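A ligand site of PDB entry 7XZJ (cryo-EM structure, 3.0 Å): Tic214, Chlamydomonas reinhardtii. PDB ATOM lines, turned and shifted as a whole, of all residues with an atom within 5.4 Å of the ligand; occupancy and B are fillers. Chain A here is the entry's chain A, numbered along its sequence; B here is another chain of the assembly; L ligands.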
ATOM      1  N   LYS A1230     -15.362  -2.582 -29.624  1.00  0.00           N
ATOM      2  CA  LYS A1230     -15.490  -3.681 -28.621  1.00  0.00           C
ATOM      3  C   LYS A1230     -16.524  -3.280 -27.573  1.00  0.00           C
ATOM      4  O   LYS A1230     -16.534  -2.106 -27.173  1.00  0.00           O
ATOM      5  CB  LYS A1230     -14.113  -4.001 -28.017  1.00  0.00           C
ATOM      6  CG  LYS A1230     -13.098  -4.543 -29.004  1.00  0.00           C
ATOM      7  CD  LYS A1230     -11.770  -4.898 -28.357  1.00  0.00           C
ATOM      8  CE  LYS A1230     -10.801  -5.545 -29.329  1.00  0.00           C
ATOM      9  NZ  LYS A1230      -9.556  -5.964 -28.652  1.00  0.00           N
ATOM     10  N   TRP A1234     -19.314  -8.298 -25.672  1.00  0.00           N
ATOM     11  CA  TRP A1234     -18.197  -8.979 -26.309  1.00  0.00           C
ATOM     12  C   TRP A1234     -17.159  -9.401 -25.274  1.00  0.00           C
ATOM     13  O   TRP A1234     -16.591 -10.502 -25.360  1.00  0.00           O
ATOM     14  CB  TRP A1234     -17.579  -8.061 -27.357  1.00  0.00           C
ATOM     15  CG  TRP A1234     -16.380  -8.594 -28.067  1.00  0.00           C
ATOM     16  CD1 TRP A1234     -16.357  -9.265 -29.257  1.00  0.00           C
ATOM     17  CD2 TRP A1234     -15.012  -8.498 -27.644  1.00  0.00           C
ATOM     18  NE1 TRP A1234     -15.067  -9.589 -29.594  1.00  0.00           N
ATOM     19  CE2 TRP A1234     -14.218  -9.129 -28.624  1.00  0.00           C
ATOM     20  CE3 TRP A1234     -14.381  -7.933 -26.530  1.00  0.00           C
ATOM     21  CZ2 TRP A1234     -12.842  -9.216 -28.518  1.00  0.00           C
ATOM     22  CZ3 TRP A1234     -13.010  -8.022 -26.433  1.00  0.00           C
ATOM     23  CH2 TRP A1234     -12.259  -8.653 -27.424  1.00  0.00           C
ATOM     24  N   TRP A1235     -16.899  -8.547 -24.286  1.00  0.00           N
ATOM     25  CA  TRP A1235     -15.949  -8.910 -23.232  1.00  0.00           C
ATOM     26  C   TRP A1235     -16.446 -10.110 -22.437  1.00  0.00           C
ATOM     27  O   TRP A1235     -15.648 -10.988 -22.068  1.00  0.00           O
ATOM     28  CB  TRP A1235     -15.709  -7.729 -22.305  1.00  0.00           C
ATOM     29  CG  TRP A1235     -14.813  -8.098 -21.162  1.00  0.00           C
ATOM     30  CD1 TRP A1235     -13.453  -8.074 -21.152  1.00  0.00           C
ATOM     31  CD2 TRP A1235     -15.221  -8.566 -19.869  1.00  0.00           C
ATOM     32  NE1 TRP A1235     -12.983  -8.496 -19.928  1.00  0.00           N
ATOM     33  CE2 TRP A1235     -14.052  -8.790 -19.126  1.00  0.00           C
ATOM     34  CE3 TRP A1235     -16.461  -8.795 -19.266  1.00  0.00           C
ATOM     35  CZ2 TRP A1235     -14.080  -9.251 -17.814  1.00  0.00           C
ATOM     36  CZ3 TRP A1235     -16.487  -9.255 -17.968  1.00  0.00           C
ATOM     37  CH2 TRP A1235     -15.310  -9.477 -17.252  1.00  0.00           C
ATOM     38  N   LYS A1238     -15.937 -13.232 -24.514  1.00  0.00           N
ATOM     39  CA  LYS A1238     -14.538 -13.643 -24.442  1.00  0.00           C
ATOM     40  C   LYS A1238     -14.197 -14.228 -23.068  1.00  0.00           C
ATOM     41  O   LYS A1238     -13.408 -15.183 -22.973  1.00  0.00           O
ATOM     42  CB  LYS A1238     -13.631 -12.456 -24.750  1.00  0.00           C
ATOM     43  CG  LYS A1238     -12.149 -12.783 -24.721  1.00  0.00           C
ATOM     44  CD  LYS A1238     -11.300 -11.535 -24.774  1.00  0.00           C
ATOM     45  CE  LYS A1238     -11.613 -10.598 -23.625  1.00  0.00           C
ATOM     46  NZ  LYS A1238     -10.767  -9.372 -23.674  1.00  0.00           N
ATOM     47  N   GLN A1239     -14.769 -13.666 -22.009  1.00  0.00           N
ATOM     48  CA  GLN A1239     -14.474 -14.137 -20.658  1.00  0.00           C
ATOM     49  C   GLN A1239     -14.909 -15.580 -20.480  1.00  0.00           C
ATOM     50  O   GLN A1239     -14.254 -16.351 -19.756  1.00  0.00           O
ATOM     51  CB  GLN A1239     -15.152 -13.229 -19.636  1.00  0.00           C
ATOM     52  CG  GLN A1239     -14.910 -13.635 -18.183  1.00  0.00           C
ATOM     53  CD  GLN A1239     -13.481 -13.358 -17.734  1.00  0.00           C
ATOM     54  OE1 GLN A1239     -12.783 -12.546 -18.331  1.00  0.00           O
ATOM     55  NE2 GLN A1239     -13.062 -14.046 -16.680  1.00  0.00           N
ATOM     56  N   ILE A1242     -12.058 -17.624 -21.558  1.00  0.00           N
ATOM     57  CA  ILE A1242     -10.897 -17.567 -20.613  1.00  0.00           C
ATOM     58  C   ILE A1242     -11.156 -18.498 -19.429  1.00  0.00           C
ATOM     59  O   ILE A1242     -10.211 -19.185 -19.003  1.00  0.00           O
ATOM     60  CB  ILE A1242     -10.644 -16.108 -20.161  1.00  0.00           C
ATOM     61  CG1 ILE A1242     -10.504 -15.166 -21.360  1.00  0.00           C
ATOM     62  CG2 ILE A1242      -9.443 -16.029 -19.241  1.00  0.00           C
ATOM     63  CD1 ILE A1242     -10.332 -13.716 -20.967  1.00  0.00           C
ATOM     64  N   GLU A1273      -2.013 -17.236 -15.696  1.00  0.00           N
ATOM     65  CA  GLU A1273      -2.664 -15.929 -15.978  1.00  0.00           C
ATOM     66  C   GLU A1273      -3.715 -15.617 -14.898  1.00  0.00           C
ATOM     67  O   GLU A1273      -3.890 -14.432 -14.592  1.00  0.00           O
ATOM     68  CB  GLU A1273      -3.284 -15.976 -17.376  1.00  0.00           C
ATOM     69  CG  GLU A1273      -4.028 -14.710 -17.774  1.00  0.00           C
ATOM     70  CD  GLU A1273      -5.537 -14.759 -17.582  1.00  0.00           C
ATOM     71  OE1 GLU A1273      -6.055 -15.856 -17.260  1.00  0.00           O
ATOM     72  OE2 GLU A1273      -6.192 -13.715 -17.752  1.00  0.00           O
ATOM     73  N   LYS A1276      -3.450 -13.043 -11.971  1.00  0.00           N
ATOM     74  CA  LYS A1276      -3.720 -11.589 -12.125  1.00  0.00           C
ATOM     75  C   LYS A1276      -4.973 -11.207 -11.333  1.00  0.00           C
ATOM     76  O   LYS A1276      -4.936 -10.152 -10.669  1.00  0.00           O
ATOM     77  CB  LYS A1276      -3.946 -11.271 -13.612  1.00  0.00           C
ATOM     78  CG  LYS A1276      -4.447  -9.872 -13.919  1.00  0.00           C
ATOM     79  CD  LYS A1276      -5.456  -9.843 -15.051  1.00  0.00           C
ATOM     80  CE  LYS A1276      -4.955 -10.531 -16.310  1.00  0.00           C
ATOM     81  NZ  LYS A1276      -5.974 -10.506 -17.378  1.00  0.00           N
ATOM     82  N   TYR A1359     -11.211  -7.477  -9.491  1.00  0.00           N
ATOM     83  CA  TYR A1359     -12.362  -6.816 -10.157  1.00  0.00           C
ATOM     84  C   TYR A1359     -13.548  -6.805  -9.187  1.00  0.00           C
ATOM     85  O   TYR A1359     -14.477  -7.610  -9.382  1.00  0.00           O
ATOM     86  CB  TYR A1359     -12.710  -7.539 -11.456  1.00  0.00           C
ATOM     87  CG  TYR A1359     -11.596  -7.620 -12.460  1.00  0.00           C
ATOM     88  CD1 TYR A1359     -10.596  -8.582 -12.354  1.00  0.00           C
ATOM     89  CD2 TYR A1359     -11.529  -6.742 -13.530  1.00  0.00           C
ATOM     90  CE1 TYR A1359      -9.561  -8.655 -13.267  1.00  0.00           C
ATOM     91  CE2 TYR A1359     -10.502  -6.806 -14.451  1.00  0.00           C
ATOM     92  CZ  TYR A1359      -9.516  -7.762 -14.327  1.00  0.00           C
ATOM     93  OH  TYR A1359      -8.501  -7.831 -15.230  1.00  0.00           O
ATOM     94  N   LYS A1457     -14.609  -5.207 -14.624  1.00  0.00           N
ATOM     95  CA  LYS A1457     -13.744  -4.721 -15.680  1.00  0.00           C
ATOM     96  C   LYS A1457     -13.968  -3.231 -15.921  1.00  0.00           C
ATOM     97  O   LYS A1457     -13.018  -2.499 -16.190  1.00  0.00           O
ATOM     98  CB  LYS A1457     -13.976  -5.497 -16.968  1.00  0.00           C
ATOM     99  CG  LYS A1457     -13.043  -5.104 -18.097  1.00  0.00           C
ATOM    100  CD  LYS A1457     -11.587  -5.192 -17.633  1.00  0.00           C
ATOM    101  CE  LYS A1457     -10.635  -4.704 -18.703  1.00  0.00           C
ATOM    102  NZ  LYS A1457     -10.677  -5.556 -19.928  1.00  0.00           N
ATOM    103  N   VAL A1460     -12.084  -1.346 -13.126  1.00  0.00           N
ATOM    104  CA  VAL A1460     -10.637  -1.344 -13.323  1.00  0.00           C
ATOM    105  C   VAL A1460     -10.260  -0.474 -14.519  1.00  0.00           C
ATOM    106  O   VAL A1460      -9.280   0.287 -14.462  1.00  0.00           O
ATOM    107  CB  VAL A1460     -10.127  -2.788 -13.488  1.00  0.00           C
ATOM    108  CG1 VAL A1460      -8.656  -2.806 -13.857  1.00  0.00           C
ATOM    109  CG2 VAL A1460     -10.360  -3.571 -12.209  1.00  0.00           C
ATOM    110  N   LYS A1464      -7.771   2.831 -14.744  1.00  0.00           N
ATOM    111  CA  LYS A1464      -6.635   2.938 -15.643  1.00  0.00           C
ATOM    112  C   LYS A1464      -6.719   4.205 -16.501  1.00  0.00           C
ATOM    113  O   LYS A1464      -5.721   4.916 -16.678  1.00  0.00           O
ATOM    114  CB  LYS A1464      -6.540   1.708 -16.532  1.00  0.00           C
ATOM    115  CG  LYS A1464      -6.395   0.399 -15.772  1.00  0.00           C
ATOM    116  CD  LYS A1464      -5.137   0.391 -14.919  1.00  0.00           C
ATOM    117  CE  LYS A1464      -5.014  -0.923 -14.158  1.00  0.00           C
ATOM    118  NZ  LYS A1464      -4.949  -2.098 -15.072  1.00  0.00           N
ATOM    119  N   ILE A1689     -12.304  -0.312 -24.007  1.00  0.00           N
ATOM    120  CA  ILE A1689     -11.151   0.208 -24.721  1.00  0.00           C
ATOM    121  C   ILE A1689      -9.863  -0.272 -24.060  1.00  0.00           C
ATOM    122  O   ILE A1689      -9.770  -0.368 -22.835  1.00  0.00           O
ATOM    123  CB  ILE A1689     -11.137   1.747 -24.859  1.00  0.00           C
ATOM    124  CG1 ILE A1689     -11.279   2.412 -23.487  1.00  0.00           C
ATOM    125  CG2 ILE A1689     -12.262   2.205 -25.780  1.00  0.00           C
ATOM    126  N   SER A1690      -8.880  -0.589 -24.894  1.00  0.00           N
ATOM    127  CA  SER A1690      -7.572  -1.026 -24.422  1.00  0.00           C
ATOM    128  C   SER A1690      -6.638   0.174 -24.252  1.00  0.00           C
ATOM    129  O   SER A1690      -6.785   1.191 -24.931  1.00  0.00           O
ATOM    130  CB  SER A1690      -6.952  -2.034 -25.388  1.00  0.00           C
ATOM    131  OG  SER A1690      -6.766  -1.460 -26.663  1.00  0.00           O
ATOM    132  N   LEU A1691      -5.664   0.039 -23.353  1.00  0.00           N
ATOM    133  CA  LEU A1691      -4.728   1.165 -23.095  1.00  0.00           C
ATOM    134  C   LEU A1691      -3.777   1.348 -24.290  1.00  0.00           C
ATOM    135  O   LEU A1691      -3.333   2.484 -24.518  1.00  0.00           O
ATOM    136  CB  LEU A1691      -3.941   0.887 -21.810  1.00  0.00           C
ATOM    137  CG  LEU A1691      -4.554   1.494 -20.537  1.00  0.00           C
ATOM    138  CD1 LEU A1691      -4.511   3.006 -20.596  1.00  0.00           C
ATOM    139  CD2 LEU A1691      -5.979   1.001 -20.331  1.00  0.00           C
ATOM    140  N   LYS A1692      -3.491   0.267 -25.027  1.00  0.00           N
ATOM    141  CA  LYS A1692      -2.533   0.375 -26.126  1.00  0.00           C
ATOM    142  C   LYS A1692      -2.989   1.355 -27.204  1.00  0.00           C
ATOM    143  O   LYS A1692      -2.143   1.918 -27.912  1.00  0.00           O
ATOM    144  CB  LYS A1692      -2.301  -0.992 -26.766  1.00  0.00           C
ATOM    145  CG  LYS A1692      -2.027  -2.109 -25.778  1.00  0.00           C
ATOM    146  CD  LYS A1692      -2.151  -3.465 -26.450  1.00  0.00           C
ATOM    147  CE  LYS A1692      -2.005  -4.585 -25.437  1.00  0.00           C
ATOM    148  NZ  LYS A1692      -2.299  -5.916 -26.041  1.00  0.00           N
ATOM    149  N   SER B 768       3.221  -3.887 -24.241  1.00  0.00           N
ATOM    150  CA  SER B 768       2.739  -4.770 -23.169  1.00  0.00           C
ATOM    151  C   SER B 768       2.928  -6.238 -23.566  1.00  0.00           C
ATOM    152  O   SER B 768       2.024  -7.057 -23.463  1.00  0.00           O
ATOM    153  CB  SER B 768       1.286  -4.457 -22.833  1.00  0.00           C
ATOM    154  OG  SER B 768       0.851  -5.215 -21.721  1.00  0.00           O
ATOM    155  N   HIS B 770       4.677  -8.695 -22.292  1.00  0.00           N
ATOM    156  CA  HIS B 770       4.644  -9.659 -21.185  1.00  0.00           C
ATOM    157  C   HIS B 770       5.467 -10.913 -21.477  1.00  0.00           C
ATOM    158  O   HIS B 770       5.127 -12.008 -21.035  1.00  0.00           O
ATOM    159  CB  HIS B 770       3.205 -10.066 -20.842  1.00  0.00           C
ATOM    160  CG  HIS B 770       2.425  -8.999 -20.139  1.00  0.00           C
ATOM    161  ND1 HIS B 770       2.553  -8.749 -18.789  1.00  0.00           N
ATOM    162  CD2 HIS B 770       1.496  -8.132 -20.595  1.00  0.00           C
ATOM    163  CE1 HIS B 770       1.747  -7.760 -18.453  1.00  0.00           C
ATOM    164  NE2 HIS B 770       1.090  -7.372 -19.524  1.00  0.00           N
ATOM    165  N   ARG B 802      -0.521  -9.412 -30.012  1.00  0.00           N
ATOM    166  CA  ARG B 802      -1.701  -9.147 -30.835  1.00  0.00           C
ATOM    167  C   ARG B 802      -1.261  -8.772 -32.239  1.00  0.00           C
ATOM    168  O   ARG B 802      -0.494  -7.821 -32.431  1.00  0.00           O
ATOM    169  CB  ARG B 802      -2.536  -8.030 -30.222  1.00  0.00           C
ATOM    170  CG  ARG B 802      -3.610  -7.506 -31.167  1.00  0.00           C
ATOM    171  CD  ARG B 802      -4.600  -6.608 -30.455  1.00  0.00           C
ATOM    172  NE  ARG B 802      -5.425  -7.339 -29.508  1.00  0.00           N
ATOM    173  CZ  ARG B 802      -6.558  -7.957 -29.818  1.00  0.00           C
ATOM    174  NH1 ARG B 802      -7.023  -7.958 -31.054  1.00  0.00           N
ATOM    175  NH2 ARG B 802      -7.226  -8.595 -28.866  1.00  0.00           N
ATOM    176  N   LYS B 807      -5.300 -12.463 -31.302  1.00  0.00           N
ATOM    177  CA  LYS B 807      -4.472 -12.387 -30.104  1.00  0.00           C
ATOM    178  C   LYS B 807      -3.845 -13.750 -29.871  1.00  0.00           C
ATOM    179  O   LYS B 807      -4.535 -14.767 -29.922  1.00  0.00           O
ATOM    180  CB  LYS B 807      -5.290 -11.945 -28.893  1.00  0.00           C
ATOM    181  CG  LYS B 807      -4.508 -11.853 -27.603  1.00  0.00           C
ATOM    182  CD  LYS B 807      -3.420 -10.800 -27.708  1.00  0.00           C
ATOM    183  CE  LYS B 807      -2.680 -10.627 -26.392  1.00  0.00           C
ATOM    184  NZ  LYS B 807      -1.587  -9.634 -26.517  1.00  0.00           N
HETATM  185  C1  LIG L   1      -6.017  -6.541 -23.206  1.00  0.00           C
HETATM  186  C2  LIG L   1      -5.143  -5.711 -22.281  1.00  0.00           C
HETATM  187  C3  LIG L   1      -5.960  -5.247 -21.097  1.00  0.00           C
HETATM  188  C4  LIG L   1      -6.496  -6.446 -20.327  1.00  0.00           C
HETATM  189  C5  LIG L   1      -7.342  -7.311 -21.240  1.00  0.00           C
HETATM  190  C6  LIG L   1      -6.557  -7.750 -22.467  1.00  0.00           C
HETATM  191  O1  LIG L   1      -5.210  -7.009 -24.327  1.00  0.00           O
HETATM  192  P1  LIG L   1      -5.661  -6.738 -25.855  1.00  0.00           P
HETATM  193  O2  LIG L   1      -4.689  -7.501 -26.736  1.00  0.00           O
HETATM  194  O3  LIG L   1      -5.558  -5.237 -26.062  1.00  0.00           O
HETATM  195  O4  LIG L   1      -7.081  -7.250 -25.995  1.00  0.00           O
HETATM  196  O5  LIG L   1      -4.070  -6.563 -21.757  1.00  0.00           O
HETATM  197  P2  LIG L   1      -2.563  -6.637 -22.335  1.00  0.00           P
HETATM  198  O6  LIG L   1      -1.797  -7.562 -21.414  1.00  0.00           O
HETATM  199  O7  LIG L   1      -2.637  -7.181 -23.751  1.00  0.00           O
HETATM  200  O8  LIG L   1      -2.027  -5.216 -22.291  1.00  0.00           O
HETATM  201  O9  LIG L   1      -5.121  -4.435 -20.220  1.00  0.00           O
HETATM  202  P3  LIG L   1      -4.719  -2.902 -20.573  1.00  0.00           P
HETATM  203  O10 LIG L   1      -3.992  -2.898 -21.911  1.00  0.00           O
HETATM  204  O11 LIG L   1      -3.818  -2.432 -19.450  1.00  0.00           O
HETATM  205  O12 LIG L   1      -6.017  -2.133 -20.628  1.00  0.00           O
HETATM  206  O13 LIG L   1      -7.311  -5.969 -19.214  1.00  0.00           O
HETATM  207  P4  LIG L   1      -6.785  -5.993 -17.686  1.00  0.00           P
HETATM  208  O14 LIG L   1      -7.838  -5.270 -16.860  1.00  0.00           O
HETATM  209  O15 LIG L   1      -6.654  -7.449 -17.304  1.00  0.00           O
HETATM  210  O16 LIG L   1      -5.449  -5.272 -17.650  1.00  0.00           O
HETATM  211  O17 LIG L   1      -7.766  -8.520 -20.508  1.00  0.00           O
HETATM  212  P5  LIG L   1      -9.239  -8.686 -19.887  1.00  0.00           P
HETATM  213  O18 LIG L   1      -9.318 -10.109 -19.357  1.00  0.00           O
HETATM  214  O19 LIG L   1     -10.219  -8.453 -21.013  1.00  0.00           O
HETATM  215  O20 LIG L   1      -9.388  -7.663 -18.782  1.00  0.00           O
HETATM  216  O21 LIG L   1      -7.451  -8.463 -23.371  1.00  0.00           O
HETATM  217  P6  LIG L   1      -7.329 -10.056 -23.636  1.00  0.00           P
HETATM  218  O22 LIG L   1      -5.868 -10.315 -23.995  1.00  0.00           O
HETATM  219  O23 LIG L   1      -8.263 -10.368 -24.782  1.00  0.00           O
HETATM  220  O24 LIG L   1      -7.730 -10.749 -22.355  1.00  0.00           O
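Merely in contact with the ligand: Leu 1691 (3.1 Å), Ser 1690 (3.6 Å) and Val 1460 (3.97 Å). Hydrophobic or aromatic side chains that line the ligand: Trp 1235, Tyr 1359, Val 1460, Leu 1691 and His 770 of chain B. Of the 20 residues printed, 14 come within 4 Å of the ligand. The nearest printed residue that does not touch the ligand is Ile 1242 (4.1 Å).
O7 of the ligand lies within salt-bridge range of NZ of Lys 1692 (2.6 Å). NZ of Lys 1457 is in salt-bridge range of O20 of the ligand, 2.7 Å away. An oxygen (O15) of the ligand is in hydrogen-bond range of the side-chain hydroxyl (OH) of Tyr 1359. The side-chain amino group of Lys 1238 is in salt-bridge range of an oxygen (O19) of the ligand (2.9 Å). An oxygen (O2) of the ligand is in salt-bridge range of the guanidinium group (NE) of Arg 802 of chain B. OG of Ser 768 of chain B is in hydrogen-bond range of O8 of the ligand, 2.9 Å away. An oxygen (O19) of the ligand is in hydrogen-bond range of the indole nitrogen (NE1) of Trp 1235 (3.0 Å). The side-chain amino group (NZ) of Lys 1276 lies within salt-bridge range of an oxygen (O15) of the ligand (3.1 Å). NE2 of His 770 of chain B sits close to O6 of the ligand (3.5 Å). The side-chain amino group of Lys 807 of chain B lies within salt-bridge range of an oxygen (O2) of the ligand (3.8 Å). O4 of the ligand is in salt-bridge range of NZ of Lys 1230 (3.9 Å).
The side-chain hydroxyl (OG) of Ser 768 of chain B is in hydrogen-bond range of a ring nitrogen (NE2) of His 770 of chain B, at 3.1 Å. OE2 of Glu 1273 lies within salt-bridge range of NZ of Lys 1276 (3.2 Å).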
